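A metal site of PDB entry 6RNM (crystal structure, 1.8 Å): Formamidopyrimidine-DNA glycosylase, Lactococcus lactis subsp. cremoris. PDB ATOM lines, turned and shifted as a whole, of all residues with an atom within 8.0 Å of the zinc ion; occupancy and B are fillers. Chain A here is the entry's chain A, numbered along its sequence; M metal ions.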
ATOM      1  N   TRP A 179       4.665  -2.597  20.569  1.00  0.00           N
ATOM      2  CA  TRP A 179       3.304  -2.679  21.078  1.00  0.00           C
ATOM      3  C   TRP A 179       3.224  -1.826  22.359  1.00  0.00           C
ATOM      4  O   TRP A 179       2.280  -1.060  22.521  1.00  0.00           O
ATOM      5  CB  TRP A 179       2.905  -4.134  21.387  1.00  0.00           C
ATOM      6  CG  TRP A 179       1.540  -4.260  21.996  1.00  0.00           C
ATOM      7  CD1 TRP A 179       0.342  -4.336  21.342  1.00  0.00           C
ATOM      8  CD2 TRP A 179       1.223  -4.289  23.404  1.00  0.00           C
ATOM      9  NE1 TRP A 179      -0.697  -4.463  22.244  1.00  0.00           N
ATOM     10  CE2 TRP A 179      -0.185  -4.381  23.512  1.00  0.00           C
ATOM     11  CE3 TRP A 179       1.981  -4.164  24.573  1.00  0.00           C
ATOM     12  CZ2 TRP A 179      -0.835  -4.454  24.750  1.00  0.00           C
ATOM     13  CZ3 TRP A 179       1.333  -4.197  25.807  1.00  0.00           C
ATOM     14  CH2 TRP A 179      -0.059  -4.337  25.880  1.00  0.00           C
ATOM     15  N   LYS A 182       3.178   1.791  21.577  1.00  0.00           N
ATOM     16  CA  LYS A 182       2.066   2.133  20.685  1.00  0.00           C
ATOM     17  C   LYS A 182       2.557   2.722  19.334  1.00  0.00           C
ATOM     18  O   LYS A 182       2.051   3.751  18.856  1.00  0.00           O
ATOM     19  CB  LYS A 182       1.073   3.073  21.402  1.00  0.00           C
ATOM     20  CG  LYS A 182       0.418   2.422  22.622  1.00  0.00           C
ATOM     21  CD  LYS A 182      -0.406   3.431  23.417  1.00  0.00           C
ATOM     22  CE  LYS A 182      -0.990   2.788  24.659  1.00  0.00           C
ATOM     23  NZ  LYS A 182      -1.782   3.750  25.467  1.00  0.00           N
ATOM     24  N   VAL A 237       2.209  -9.664  22.289  1.00  0.00           N
ATOM     25  CA  VAL A 237       1.979  -9.740  20.850  1.00  0.00           C
ATOM     26  C   VAL A 237       2.748 -10.845  20.140  1.00  0.00           C
ATOM     27  O   VAL A 237       2.187 -11.438  19.219  1.00  0.00           O
ATOM     28  CB  VAL A 237       2.227  -8.388  20.102  1.00  0.00           C
ATOM     29  CG1 VAL A 237       1.111  -7.398  20.357  1.00  0.00           C
ATOM     30  CG2 VAL A 237       3.599  -7.781  20.426  1.00  0.00           C
ATOM     31  N   LYS A 244      -6.556 -11.725  21.356  1.00  0.00           N
ATOM     32  CA  LYS A 244      -6.968 -10.342  21.624  1.00  0.00           C
ATOM     33  C   LYS A 244      -5.896  -9.545  22.339  1.00  0.00           C
ATOM     34  O   LYS A 244      -5.162 -10.066  23.188  1.00  0.00           O
ATOM     35  CB  LYS A 244      -8.296 -10.324  22.406  1.00  0.00           C
ATOM     36  CG  LYS A 244      -9.470 -10.891  21.604  1.00  0.00           C
ATOM     37  N   CYS A 245      -5.778  -8.257  21.959  1.00  0.00           N
ATOM     38  CA  CYS A 245      -4.880  -7.291  22.578  1.00  0.00           C
ATOM     39  C   CYS A 245      -5.336  -7.092  24.017  1.00  0.00           C
ATOM     40  O   CYS A 245      -6.529  -6.862  24.244  1.00  0.00           O
ATOM     41  CB  CYS A 245      -4.926  -5.967  21.810  1.00  0.00           C
ATOM     42  SG  CYS A 245      -4.046  -4.619  22.629  1.00  0.00           S
ATOM     43  N   SER A 246      -4.425  -7.144  24.990  1.00  0.00           N
ATOM     44  CA  SER A 246      -4.797  -6.963  26.400  1.00  0.00           C
ATOM     45  C   SER A 246      -5.312  -5.534  26.729  1.00  0.00           C
ATOM     46  O   SER A 246      -6.025  -5.370  27.709  1.00  0.00           O
ATOM     47  CB  SER A 246      -3.637  -7.325  27.316  1.00  0.00           C
ATOM     48  OG  SER A 246      -2.566  -6.428  27.084  1.00  0.00           O
ATOM     49  N   ARG A 247      -4.966  -4.528  25.890  1.00  0.00           N
ATOM     50  CA  ARG A 247      -5.431  -3.155  26.129  1.00  0.00           C
ATOM     51  C   ARG A 247      -6.792  -2.821  25.546  1.00  0.00           C
ATOM     52  O   ARG A 247      -7.643  -2.276  26.255  1.00  0.00           O
ATOM     53  CB  ARG A 247      -4.401  -2.115  25.638  1.00  0.00           C
ATOM     54  CG  ARG A 247      -3.201  -1.944  26.562  1.00  0.00           C
ATOM     55  CD  ARG A 247      -2.263  -0.833  26.091  1.00  0.00           C
ATOM     56  NE  ARG A 247      -1.878  -1.060  24.701  1.00  0.00           N
ATOM     57  CZ  ARG A 247      -0.643  -0.944  24.215  1.00  0.00           C
ATOM     58  NH1 ARG A 247       0.361  -0.576  25.001  1.00  0.00           N
ATOM     59  NH2 ARG A 247      -0.403  -1.198  22.939  1.00  0.00           N
ATOM     60  N   CYS A 248      -6.991  -3.107  24.261  1.00  0.00           N
ATOM     61  CA  CYS A 248      -8.198  -2.704  23.547  1.00  0.00           C
ATOM     62  C   CYS A 248      -9.120  -3.842  23.160  1.00  0.00           C
ATOM     63  O   CYS A 248     -10.285  -3.576  22.876  1.00  0.00           O
ATOM     64  CB  CYS A 248      -7.817  -1.883  22.314  1.00  0.00           C
ATOM     65  SG  CYS A 248      -7.089  -2.856  20.982  1.00  0.00           S
ATOM     66  N   GLY A 249      -8.602  -5.070  23.079  1.00  0.00           N
ATOM     67  CA  GLY A 249      -9.402  -6.223  22.683  1.00  0.00           C
ATOM     68  C   GLY A 249      -9.454  -6.521  21.202  1.00  0.00           C
ATOM     69  O   GLY A 249     -10.130  -7.466  20.806  1.00  0.00           O
ATOM     70  N   ALA A 250      -8.731  -5.747  20.354  1.00  0.00           N
ATOM     71  CA  ALA A 250      -8.688  -6.053  18.907  1.00  0.00           C
ATOM     72  C   ALA A 250      -7.798  -7.295  18.708  1.00  0.00           C
ATOM     73  O   ALA A 250      -6.928  -7.546  19.543  1.00  0.00           O
ATOM     74  CB  ALA A 250      -8.103  -4.875  18.142  1.00  0.00           C
ATOM     75  N   GLU A 251      -7.986  -8.067  17.620  1.00  0.00           N
ATOM     76  CA  GLU A 251      -7.128  -9.221  17.331  1.00  0.00           C
ATOM     77  C   GLU A 251      -5.738  -8.778  16.908  1.00  0.00           C
ATOM     78  O   GLU A 251      -5.594  -7.870  16.092  1.00  0.00           O
ATOM     79  CB  GLU A 251      -7.683 -10.113  16.217  1.00  0.00           C
ATOM     80  CG  GLU A 251      -8.780 -11.031  16.698  1.00  0.00           C
ATOM     81  CD  GLU A 251      -9.191 -12.125  15.726  1.00  0.00           C
ATOM     82  OE1 GLU A 251      -8.536 -12.312  14.674  1.00  0.00           O
ATOM     83  OE2 GLU A 251     -10.181 -12.822  16.054  1.00  0.00           O
ATOM     84  N   ILE A 252      -4.725  -9.474  17.428  1.00  0.00           N
ATOM     85  CA  ILE A 252      -3.343  -9.237  17.035  1.00  0.00           C
ATOM     86  C   ILE A 252      -3.198  -9.773  15.610  1.00  0.00           C
ATOM     87  O   ILE A 252      -3.660 -10.881  15.300  1.00  0.00           O
ATOM     88  CB  ILE A 252      -2.366  -9.933  18.032  1.00  0.00           C
ATOM     89  CG1 ILE A 252      -2.556  -9.416  19.489  1.00  0.00           C
ATOM     90  CG2 ILE A 252      -0.895  -9.862  17.572  1.00  0.00           C
ATOM     91  CD1 ILE A 252      -2.519  -7.829  19.687  1.00  0.00           C
ATOM     92  N   PHE A 264       1.420  -7.275  15.763  1.00  0.00           N
ATOM     93  CA  PHE A 264       1.058  -5.952  16.270  1.00  0.00           C
ATOM     94  C   PHE A 264      -0.441  -5.819  16.457  1.00  0.00           C
ATOM     95  O   PHE A 264      -1.207  -6.582  15.866  1.00  0.00           O
ATOM     96  CB  PHE A 264       1.592  -4.858  15.272  1.00  0.00           C
ATOM     97  CG  PHE A 264       0.768  -4.745  13.996  1.00  0.00           C
ATOM     98  CD1 PHE A 264       0.828  -5.728  13.016  1.00  0.00           C
ATOM     99  CD2 PHE A 264      -0.094  -3.667  13.806  1.00  0.00           C
ATOM    100  CE1 PHE A 264       0.033  -5.648  11.874  1.00  0.00           C
ATOM    101  CE2 PHE A 264      -0.889  -3.587  12.663  1.00  0.00           C
ATOM    102  CZ  PHE A 264      -0.821  -4.585  11.711  1.00  0.00           C
ATOM    103  N   CYS A 265      -0.859  -4.826  17.272  1.00  0.00           N
ATOM    104  CA  CYS A 265      -2.271  -4.520  17.453  1.00  0.00           C
ATOM    105  C   CYS A 265      -2.586  -3.357  16.484  1.00  0.00           C
ATOM    106  O   CYS A 265      -2.005  -2.276  16.648  1.00  0.00           O
ATOM    107  CB  CYS A 265      -2.606  -4.133  18.888  1.00  0.00           C
ATOM    108  SG  CYS A 265      -4.297  -3.483  19.057  1.00  0.00           S
ATOM    109  N   PRO A 266      -3.507  -3.538  15.514  1.00  0.00           N
ATOM    110  CA  PRO A 266      -3.838  -2.449  14.580  1.00  0.00           C
ATOM    111  C   PRO A 266      -4.532  -1.240  15.200  1.00  0.00           C
ATOM    112  O   PRO A 266      -4.530  -0.189  14.591  1.00  0.00           O
ATOM    113  CB  PRO A 266      -4.758  -3.100  13.547  1.00  0.00           C
ATOM    114  CG  PRO A 266      -4.715  -4.548  13.816  1.00  0.00           C
ATOM    115  CD  PRO A 266      -4.300  -4.757  15.222  1.00  0.00           C
ATOM    116  N   VAL A 267      -5.142  -1.394  16.390  1.00  0.00           N
ATOM    117  CA  VAL A 267      -5.820  -0.253  17.046  1.00  0.00           C
ATOM    118  C   VAL A 267      -4.763   0.581  17.804  1.00  0.00           C
ATOM    119  O   VAL A 267      -4.690   1.797  17.628  1.00  0.00           O
ATOM    120  CB  VAL A 267      -6.966  -0.727  17.971  1.00  0.00           C
ATOM    121  CG1 VAL A 267      -7.458   0.406  18.877  1.00  0.00           C
ATOM    122  CG2 VAL A 267      -8.136  -1.261  17.142  1.00  0.00           C
ATOM    123  N   CYS A 268      -4.004  -0.088  18.672  1.00  0.00           N
ATOM    124  CA  CYS A 268      -2.978   0.512  19.525  1.00  0.00           C
ATOM    125  C   CYS A 268      -1.790   1.051  18.747  1.00  0.00           C
ATOM    126  O   CYS A 268      -1.146   1.992  19.205  1.00  0.00           O
ATOM    127  CB  CYS A 268      -2.528  -0.497  20.576  1.00  0.00           C
ATOM    128  SG  CYS A 268      -3.812  -0.891  21.802  1.00  0.00           S
ATOM    129  N   GLN A 269      -1.486   0.446  17.601  1.00  0.00           N
ATOM    130  CA  GLN A 269      -0.324   0.810  16.789  1.00  0.00           C
ATOM    131  C   GLN A 269      -0.790   1.302  15.439  1.00  0.00           C
ATOM    132  O   GLN A 269      -0.700   0.592  14.446  1.00  0.00           O
ATOM    133  CB  GLN A 269       0.671  -0.365  16.666  1.00  0.00           C
ATOM    134  CG  GLN A 269       1.235  -0.820  18.014  1.00  0.00           C
ATOM    135  CD  GLN A 269       1.862  -2.183  17.917  1.00  0.00           C
ATOM    136  OE1 GLN A 269       1.253  -3.204  18.304  1.00  0.00           O
ATOM    137  NE2 GLN A 269       3.104  -2.252  17.438  1.00  0.00           N
HETATM  138 ZN    ZN M   1      -4.762  -2.887  21.174  1.00  0.00          ZN
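The backbone NH (N) of Val 267 sits close to the side-chain sulfur (SG) of Cys 265, at 3.5 Å. The backbone NH (N) of Cys 265 sits at hydrogen-bond distance from the side-chain amide oxygen (OE1) of Gln 269, at 2.9 Å. The side-chain sulfur (SG) of Cys 268 lies close to the guanidinium group (NE) of Arg 247. The backbone NH (N) of Ala 250 lies close to the side-chain sulfur (SG) of Cys 248 (3.4 Å). SG of Cys 245 sits close to NE1 of Trp 179 (3.4 Å). The side-chain sulfur of Cys 245 sits close to the backbone NH of Arg 247 (3.4 Å). O of Ala 250 lies within hydrogen-bond range of N of Cys 245 (2.8 Å).
Four residues have an atom within 4 Å of the zinc ion: Cys 245, Cys 248, Cys 265 and Cys 268.
The zinc ion is bound by SG of Cys 265 (2.2 Å), SG of Cys 268 (2.3 Å), SG of Cys 248 (2.3 Å) and SG of Cys 245 (2.4 Å).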
